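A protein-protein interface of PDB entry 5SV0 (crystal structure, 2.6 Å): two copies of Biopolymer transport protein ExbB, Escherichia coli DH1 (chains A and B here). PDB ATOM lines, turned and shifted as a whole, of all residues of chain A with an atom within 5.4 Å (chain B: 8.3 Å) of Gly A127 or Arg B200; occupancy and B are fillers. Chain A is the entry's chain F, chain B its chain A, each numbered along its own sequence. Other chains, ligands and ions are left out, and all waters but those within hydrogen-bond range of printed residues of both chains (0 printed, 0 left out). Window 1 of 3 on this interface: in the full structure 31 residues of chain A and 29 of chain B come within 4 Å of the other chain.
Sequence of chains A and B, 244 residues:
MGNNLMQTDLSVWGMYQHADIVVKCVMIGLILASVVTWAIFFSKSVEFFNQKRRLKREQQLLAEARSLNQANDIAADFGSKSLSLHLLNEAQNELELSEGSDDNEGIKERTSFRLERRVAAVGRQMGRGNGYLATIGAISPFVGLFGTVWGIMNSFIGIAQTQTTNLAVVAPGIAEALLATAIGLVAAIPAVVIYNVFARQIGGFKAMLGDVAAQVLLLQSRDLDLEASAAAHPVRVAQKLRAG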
ATOM      1  N   VAL A 122       3.894  22.613 -14.664  1.00  0.00           N
ATOM      2  CA  VAL A 122       3.617  23.955 -15.170  1.00  0.00           C
ATOM      3  C   VAL A 122       3.044  23.861 -16.572  1.00  0.00           C
ATOM      4  O   VAL A 122       2.037  24.505 -16.894  1.00  0.00           O
ATOM      5  CB  VAL A 122       4.880  24.830 -15.122  1.00  0.00           C
ATOM      6  CG1 VAL A 122       4.660  26.124 -15.816  1.00  0.00           C
ATOM      7  CG2 VAL A 122       5.226  25.131 -13.713  1.00  0.00           C
ATOM      8  N   GLY A 123       3.614  22.982 -17.397  1.00  0.00           N
ATOM      9  CA  GLY A 123       3.057  22.796 -18.717  1.00  0.00           C
ATOM     10  C   GLY A 123       1.604  22.400 -18.642  1.00  0.00           C
ATOM     11  O   GLY A 123       0.749  22.993 -19.300  1.00  0.00           O
ATOM     12  N   ARG A 124       1.291  21.461 -17.752  1.00  0.00           N
ATOM     13  CA  ARG A 124      -0.089  21.015 -17.625  1.00  0.00           C
ATOM     14  C   ARG A 124      -0.975  22.158 -17.191  1.00  0.00           C
ATOM     15  O   ARG A 124      -2.064  22.343 -17.741  1.00  0.00           O
ATOM     16  CB  ARG A 124      -0.191  19.859 -16.641  1.00  0.00           C
ATOM     17  CG  ARG A 124      -0.320  18.490 -17.279  1.00  0.00           C
ATOM     18  CD  ARG A 124      -0.689  17.458 -16.225  1.00  0.00           C
ATOM     19  NE  ARG A 124       0.209  17.534 -15.068  1.00  0.00           N
ATOM     20  CZ  ARG A 124       1.427  16.985 -15.005  1.00  0.00           C
ATOM     21  NH1 ARG A 124       1.923  16.305 -16.039  1.00  0.00           N
ATOM     22  NH2 ARG A 124       2.159  17.124 -13.905  1.00  0.00           N
ATOM     23  N   GLN A 125      -0.489  22.982 -16.255  1.00  0.00           N
ATOM     24  CA  GLN A 125      -1.304  24.091 -15.762  1.00  0.00           C
ATOM     25  C   GLN A 125      -1.548  25.128 -16.838  1.00  0.00           C
ATOM     26  O   GLN A 125      -2.550  25.844 -16.786  1.00  0.00           O
ATOM     27  CB  GLN A 125      -0.644  24.779 -14.574  1.00  0.00           C
ATOM     28  CG  GLN A 125      -0.416  23.923 -13.376  1.00  0.00           C
ATOM     29  CD  GLN A 125       0.570  24.575 -12.444  1.00  0.00           C
ATOM     30  OE1 GLN A 125       0.709  25.800 -12.443  1.00  0.00           O
ATOM     31  NE2 GLN A 125       1.284  23.768 -11.663  1.00  0.00           N
ATOM     32  N   MET A 126      -0.631  25.263 -17.790  1.00  0.00           N
ATOM     33  CA  MET A 126      -0.919  26.186 -18.874  1.00  0.00           C
ATOM     34  C   MET A 126      -1.805  25.538 -19.927  1.00  0.00           C
ATOM     35  O   MET A 126      -2.572  26.239 -20.591  1.00  0.00           O
ATOM     36  CB  MET A 126       0.376  26.701 -19.490  1.00  0.00           C
ATOM     37  CG  MET A 126       1.361  27.246 -18.469  1.00  0.00           C
ATOM     38  SD  MET A 126       2.523  28.394 -19.235  1.00  0.00           S
ATOM     39  CE  MET A 126       2.418  27.883 -20.951  1.00  0.00           C
ATOM     40  N   GLY A 127      -1.739  24.209 -20.071  1.00  0.00           N
ATOM     41  CA  GLY A 127      -2.621  23.531 -20.998  1.00  0.00           C
ATOM     42  C   GLY A 127      -4.073  23.622 -20.608  1.00  0.00           C
ATOM     43  O   GLY A 127      -4.941  23.165 -21.360  1.00  0.00           O
ATOM     44  N   ARG A 128      -4.334  24.200 -19.441  1.00  0.00           N
ATOM     45  CA  ARG A 128      -5.675  24.356 -18.914  1.00  0.00           C
ATOM     46  C   ARG A 128      -6.426  25.423 -19.696  1.00  0.00           C
ATOM     47  O   ARG A 128      -5.942  26.540 -19.880  1.00  0.00           O
ATOM     48  CB  ARG A 128      -5.583  24.730 -17.441  1.00  0.00           C
ATOM     49  CG  ARG A 128      -6.894  24.885 -16.725  1.00  0.00           C
ATOM     50  CD  ARG A 128      -6.635  25.478 -15.347  1.00  0.00           C
ATOM     51  NE  ARG A 128      -5.390  24.954 -14.781  1.00  0.00           N
ATOM     52  CZ  ARG A 128      -4.676  25.551 -13.827  1.00  0.00           C
ATOM     53  NH1 ARG A 128      -5.070  26.712 -13.313  1.00  0.00           N
ATOM     54  NH2 ARG A 128      -3.557  24.987 -13.385  1.00  0.00           N
ATOM     55  N   GLY A 129      -7.616  25.080 -20.151  1.00  0.00           N
ATOM     56  CA  GLY A 129      -8.423  25.973 -20.927  1.00  0.00           C
ATOM     57  C   GLY A 129      -8.197  25.859 -22.416  1.00  0.00           C
ATOM     58  O   GLY A 129      -9.107  26.164 -23.197  1.00  0.00           O
ATOM     59  N   ASN A 130      -7.015  25.399 -22.834  1.00  0.00           N
ATOM     60  CA  ASN A 130      -6.840  25.083 -24.240  1.00  0.00           C
ATOM     61  C   ASN A 130      -7.737  23.913 -24.636  1.00  0.00           C
ATOM     62  O   ASN A 130      -8.090  23.757 -25.813  1.00  0.00           O
ATOM     63  CB  ASN A 130      -5.375  24.798 -24.547  1.00  0.00           C
ATOM     64  CG  ASN A 130      -4.925  25.442 -25.851  1.00  0.00           C
ATOM     65  OD1 ASN A 130      -5.592  26.331 -26.376  1.00  0.00           O
ATOM     66  ND2 ASN A 130      -3.806  24.984 -26.388  1.00  0.00           N
ATOM     67  N   GLY A 131      -8.104  23.074 -23.668  1.00  0.00           N
ATOM     68  CA  GLY A 131      -9.030  22.000 -23.961  1.00  0.00           C
ATOM     69  C   GLY A 131     -10.339  22.510 -24.518  1.00  0.00           C
ATOM     70  O   GLY A 131     -10.841  21.986 -25.509  1.00  0.00           O
ATOM     71  N   ILE A 202       2.721  27.120 -25.658  1.00  0.00           N
ATOM     72  CA  ILE A 202       2.909  26.306 -24.462  1.00  0.00           C
ATOM     73  C   ILE A 202       4.094  25.391 -24.631  1.00  0.00           C
ATOM     74  O   ILE A 202       4.899  25.215 -23.702  1.00  0.00           O
ATOM     75  CB  ILE A 202       1.641  25.502 -24.137  1.00  0.00           C
ATOM     76  CG1 ILE A 202       0.552  26.421 -23.567  1.00  0.00           C
ATOM     77  CG2 ILE A 202       1.943  24.389 -23.187  1.00  0.00           C
ATOM     78  CD1 ILE A 202      -0.785  25.728 -23.402  1.00  0.00           C
ATOM     79  N   PHE B  48     -15.433   8.249 -10.941  1.00  0.00           N
ATOM     80  CA  PHE B  48     -14.240   9.076 -11.051  1.00  0.00           C
ATOM     81  C   PHE B  48     -14.205  10.136  -9.964  1.00  0.00           C
ATOM     82  O   PHE B  48     -13.151  10.374  -9.361  1.00  0.00           O
ATOM     83  CB  PHE B  48     -14.144   9.734 -12.425  1.00  0.00           C
ATOM     84  CG  PHE B  48     -12.998  10.692 -12.529  1.00  0.00           C
ATOM     85  CD1 PHE B  48     -11.706  10.223 -12.729  1.00  0.00           C
ATOM     86  CD2 PHE B  48     -13.194  12.058 -12.372  1.00  0.00           C
ATOM     87  CE1 PHE B  48     -10.628  11.105 -12.803  1.00  0.00           C
ATOM     88  CE2 PHE B  48     -12.124  12.947 -12.440  1.00  0.00           C
ATOM     89  CZ  PHE B  48     -10.837  12.468 -12.654  1.00  0.00           C
ATOM     90  N   LYS B  52     -11.189  10.424  -7.239  1.00  0.00           N
ATOM     91  CA  LYS B  52     -10.383  11.640  -7.285  1.00  0.00           C
ATOM     92  C   LYS B  52     -10.341  12.358  -5.927  1.00  0.00           C
ATOM     93  O   LYS B  52      -9.299  12.916  -5.542  1.00  0.00           O
ATOM     94  CB  LYS B  52     -10.904  12.585  -8.365  1.00  0.00           C
ATOM     95  CG  LYS B  52     -10.021  13.829  -8.501  1.00  0.00           C
ATOM     96  CD  LYS B  52     -10.348  14.725  -9.683  1.00  0.00           C
ATOM     97  CE  LYS B  52      -9.595  16.047  -9.552  1.00  0.00           C
ATOM     98  NZ  LYS B  52     -10.050  17.086 -10.525  1.00  0.00           N
ATOM     99  N   VAL B 193     -17.882  15.305 -26.778  1.00  0.00           N
ATOM    100  CA  VAL B 193     -17.609  16.190 -25.654  1.00  0.00           C
ATOM    101  C   VAL B 193     -17.329  15.388 -24.387  1.00  0.00           C
ATOM    102  O   VAL B 193     -16.300  15.587 -23.727  1.00  0.00           O
ATOM    103  CB  VAL B 193     -18.756  17.184 -25.453  1.00  0.00           C
ATOM    104  CG1 VAL B 193     -18.659  17.813 -24.057  1.00  0.00           C
ATOM    105  CG2 VAL B 193     -18.679  18.235 -26.531  1.00  0.00           C
ATOM    106  N   ILE B 194     -18.236  14.473 -24.029  1.00  0.00           N
ATOM    107  CA  ILE B 194     -18.012  13.607 -22.873  1.00  0.00           C
ATOM    108  C   ILE B 194     -16.649  12.945 -22.947  1.00  0.00           C
ATOM    109  O   ILE B 194     -15.904  12.906 -21.960  1.00  0.00           O
ATOM    110  CB  ILE B 194     -19.117  12.543 -22.779  1.00  0.00           C
ATOM    111  CG1 ILE B 194     -20.437  13.162 -22.328  1.00  0.00           C
ATOM    112  CG2 ILE B 194     -18.686  11.425 -21.860  1.00  0.00           C
ATOM    113  CD1 ILE B 194     -21.624  12.202 -22.390  1.00  0.00           C
ATOM    114  N   TYR B 195     -16.288  12.446 -24.126  1.00  0.00           N
ATOM    115  CA  TYR B 195     -14.986  11.818 -24.305  1.00  0.00           C
ATOM    116  C   TYR B 195     -13.843  12.773 -23.977  1.00  0.00           C
ATOM    117  O   TYR B 195     -12.855  12.376 -23.349  1.00  0.00           O
ATOM    118  CB  TYR B 195     -14.849  11.324 -25.732  1.00  0.00           C
ATOM    119  CG  TYR B 195     -13.488  10.785 -25.994  1.00  0.00           C
ATOM    120  CD1 TYR B 195     -13.231   9.447 -25.799  1.00  0.00           C
ATOM    121  CD2 TYR B 195     -12.451  11.611 -26.416  1.00  0.00           C
ATOM    122  CE1 TYR B 195     -11.997   8.928 -26.024  1.00  0.00           C
ATOM    123  CE2 TYR B 195     -11.203  11.100 -26.639  1.00  0.00           C
ATOM    124  CZ  TYR B 195     -10.984   9.746 -26.442  1.00  0.00           C
ATOM    125  OH  TYR B 195      -9.749   9.181 -26.659  1.00  0.00           O
ATOM    126  N   ASN B 196     -13.932  14.020 -24.444  1.00  0.00           N
ATOM    127  CA  ASN B 196     -12.867  14.968 -24.153  1.00  0.00           C
ATOM    128  C   ASN B 196     -12.770  15.217 -22.655  1.00  0.00           C
ATOM    129  O   ASN B 196     -11.671  15.211 -22.087  1.00  0.00           O
ATOM    130  CB  ASN B 196     -13.092  16.262 -24.927  1.00  0.00           C
ATOM    131  CG  ASN B 196     -12.705  16.114 -26.382  1.00  0.00           C
ATOM    132  OD1 ASN B 196     -12.435  14.991 -26.840  1.00  0.00           O
ATOM    133  ND2 ASN B 196     -12.673  17.225 -27.119  1.00  0.00           N
ATOM    134  N   VAL B 197     -13.915  15.391 -21.992  1.00  0.00           N
ATOM    135  CA  VAL B 197     -13.914  15.583 -20.544  1.00  0.00           C
ATOM    136  C   VAL B 197     -13.229  14.417 -19.846  1.00  0.00           C
ATOM    137  O   VAL B 197     -12.428  14.607 -18.922  1.00  0.00           O
ATOM    138  CB  VAL B 197     -15.348  15.754 -20.024  1.00  0.00           C
ATOM    139  CG1 VAL B 197     -15.315  16.215 -18.585  1.00  0.00           C
ATOM    140  CG2 VAL B 197     -16.101  16.739 -20.888  1.00  0.00           C
ATOM    141  N   PHE B 198     -13.543  13.189 -20.259  1.00  0.00           N
ATOM    142  CA  PHE B 198     -12.922  12.042 -19.607  1.00  0.00           C
ATOM    143  C   PHE B 198     -11.434  11.989 -19.895  1.00  0.00           C
ATOM    144  O   PHE B 198     -10.659  11.555 -19.041  1.00  0.00           O
ATOM    145  CB  PHE B 198     -13.596  10.738 -20.022  1.00  0.00           C
ATOM    146  CG  PHE B 198     -14.953  10.548 -19.400  1.00  0.00           C
ATOM    147  CD1 PHE B 198     -15.456  11.492 -18.507  1.00  0.00           C
ATOM    148  CD2 PHE B 198     -15.725   9.432 -19.698  1.00  0.00           C
ATOM    149  CE1 PHE B 198     -16.711  11.343 -17.948  1.00  0.00           C
ATOM    150  CE2 PHE B 198     -16.970   9.268 -19.133  1.00  0.00           C
ATOM    151  CZ  PHE B 198     -17.469  10.231 -18.258  1.00  0.00           C
ATOM    152  N   ALA B 199     -11.014  12.403 -21.088  1.00  0.00           N
ATOM    153  CA  ALA B 199      -9.585  12.443 -21.369  1.00  0.00           C
ATOM    154  C   ALA B 199      -8.872  13.423 -20.436  1.00  0.00           C
ATOM    155  O   ALA B 199      -7.810  13.108 -19.888  1.00  0.00           O
ATOM    156  CB  ALA B 199      -9.349  12.810 -22.835  1.00  0.00           C
ATOM    157  N   ARG B 200      -9.452  14.608 -20.230  1.00  0.00           N
ATOM    158  CA  ARG B 200      -8.851  15.588 -19.329  1.00  0.00           C
ATOM    159  C   ARG B 200      -8.780  15.050 -17.907  1.00  0.00           C
ATOM    160  O   ARG B 200      -7.718  15.068 -17.265  1.00  0.00           O
ATOM    161  CB  ARG B 200      -9.665  16.882 -19.355  1.00  0.00           C
ATOM    162  CG  ARG B 200      -8.856  18.150 -19.369  1.00  0.00           C
ATOM    163  CD  ARG B 200      -8.308  18.415 -20.757  1.00  0.00           C
ATOM    164  NE  ARG B 200      -7.551  19.662 -20.807  1.00  0.00           N
ATOM    165  CZ  ARG B 200      -6.979  20.146 -21.904  1.00  0.00           C
ATOM    166  NH1 ARG B 200      -7.079  19.489 -23.051  1.00  0.00           N
ATOM    167  NH2 ARG B 200      -6.310  21.291 -21.855  1.00  0.00           N
ATOM    168  N   GLN B 201      -9.915  14.580 -17.395  1.00  0.00           N
ATOM    169  CA  GLN B 201      -9.981  14.131 -16.013  1.00  0.00           C
ATOM    170  C   GLN B 201      -9.063  12.945 -15.766  1.00  0.00           C
ATOM    171  O   GLN B 201      -8.419  12.846 -14.710  1.00  0.00           O
ATOM    172  CB  GLN B 201     -11.411  13.771 -15.668  1.00  0.00           C
ATOM    173  CG  GLN B 201     -12.347  14.920 -15.707  1.00  0.00           C
ATOM    174  CD  GLN B 201     -13.695  14.513 -15.182  1.00  0.00           C
ATOM    175  OE1 GLN B 201     -14.244  13.489 -15.595  1.00  0.00           O
ATOM    176  NE2 GLN B 201     -14.227  15.286 -14.243  1.00  0.00           N
ATOM    177  N   ILE B 202      -9.030  12.011 -16.705  1.00  0.00           N
ATOM    178  CA  ILE B 202      -8.119  10.880 -16.588  1.00  0.00           C
ATOM    179  C   ILE B 202      -6.676  11.353 -16.575  1.00  0.00           C
ATOM    180  O   ILE B 202      -5.875  10.898 -15.753  1.00  0.00           O
ATOM    181  CB  ILE B 202      -8.391   9.876 -17.715  1.00  0.00           C
ATOM    182  CG1 ILE B 202      -9.685   9.128 -17.411  1.00  0.00           C
ATOM    183  CG2 ILE B 202      -7.235   8.952 -17.904  1.00  0.00           C
ATOM    184  CD1 ILE B 202     -10.137   8.296 -18.531  1.00  0.00           C
ATOM    185  N   GLY B 203      -6.334  12.312 -17.439  1.00  0.00           N
ATOM    186  CA  GLY B 203      -4.983  12.849 -17.425  1.00  0.00           C
ATOM    187  C   GLY B 203      -4.596  13.381 -16.059  1.00  0.00           C
ATOM    188  O   GLY B 203      -3.519  13.066 -15.532  1.00  0.00           O
ATOM    189  N   GLY B 204      -5.487  14.159 -15.445  1.00  0.00           N
ATOM    190  CA  GLY B 204      -5.193  14.693 -14.125  1.00  0.00           C
ATOM    191  C   GLY B 204      -5.067  13.616 -13.065  1.00  0.00           C
ATOM    192  O   GLY B 204      -4.213  13.703 -12.174  1.00  0.00           O
ATOM    193  N   PHE B 205      -5.903  12.573 -13.154  1.00  0.00           N
ATOM    194  CA  PHE B 205      -5.819  11.488 -12.181  1.00  0.00           C
ATOM    195  C   PHE B 205      -4.482  10.760 -12.308  1.00  0.00           C
ATOM    196  O   PHE B 205      -3.816  10.466 -11.310  1.00  0.00           O
ATOM    197  CB  PHE B 205      -6.979  10.518 -12.388  1.00  0.00           C
ATOM    198  CG  PHE B 205      -7.173   9.518 -11.254  1.00  0.00           C
ATOM    199  CD1 PHE B 205      -6.447   8.320 -11.197  1.00  0.00           C
ATOM    200  CD2 PHE B 205      -8.113   9.776 -10.248  1.00  0.00           C
ATOM    201  CE1 PHE B 205      -6.646   7.415 -10.150  1.00  0.00           C
ATOM    202  CE2 PHE B 205      -8.315   8.874  -9.202  1.00  0.00           C
ATOM    203  CZ  PHE B 205      -7.580   7.696  -9.147  1.00  0.00           C
ATOM    204  N   LYS B 206      -4.078  10.460 -13.538  1.00  0.00           N
ATOM    205  CA  LYS B 206      -2.763   9.886 -13.773  1.00  0.00           C
ATOM    206  C   LYS B 206      -1.670  10.742 -13.152  1.00  0.00           C
ATOM    207  O   LYS B 206      -0.745  10.224 -12.517  1.00  0.00           O
ATOM    208  CB  LYS B 206      -2.529   9.736 -15.273  1.00  0.00           C
ATOM    209  CG  LYS B 206      -3.354   8.679 -15.964  1.00  0.00           C
ATOM    210  CD  LYS B 206      -3.070   8.756 -17.445  1.00  0.00           C
ATOM    211  CE  LYS B 206      -3.858   7.747 -18.239  1.00  0.00           C
ATOM    212  NZ  LYS B 206      -3.294   7.628 -19.600  1.00  0.00           N
ATOM    213  N   ALA B 207      -1.746  12.061 -13.331  1.00  0.00           N
ATOM    214  CA  ALA B 207      -0.728  12.914 -12.725  1.00  0.00           C
ATOM    215  C   ALA B 207      -0.724  12.771 -11.198  1.00  0.00           C
ATOM    216  O   ALA B 207       0.332  12.600 -10.586  1.00  0.00           O
ATOM    217  CB  ALA B 207      -0.928  14.364 -13.164  1.00  0.00           C
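O of Gly A127 sits close to NH2 of Arg B200 (2.4 Å). N of Gly A131 sits close to NH2 of Arg B200 (3.1 Å).
Among the printed residues, pairs that only touch across the chains: Arg A124 with Ala B207 (3.9 Å).
Of chain B, only Arg B200 (2.4 Å) comes within 4 Å of Gly A127. Arg B200 touches two residues of chain A. Printed residues of chain B within 4 Å of Gly A131: Arg B200 (3.1 Å). Of the printed residues of chain B, Arg A124 touches Ala B207 (3.9 Å). Of the printed residues of chain A, Ala B207 touches Arg A124 (3.9 Å). The nearest residue of chain A that does not touch Arg B200 is Asn A130 (4.1 Å).
Hydrophobic or aromatic side chains of chain B within 4 Å of the printed part of chain A: Ala B207. Among the printed residues, 3 pairs touch across the chains. Among the printed residues, no Asp or Glu carboxylate lies within 4 Å of a Lys or Arg side-chain nitrogen of the other chain.
Position printed for both chains: 202. Of the 3 pairs that touch across the chains among the printed residues, none has its exchanged pair printed and touching as well.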
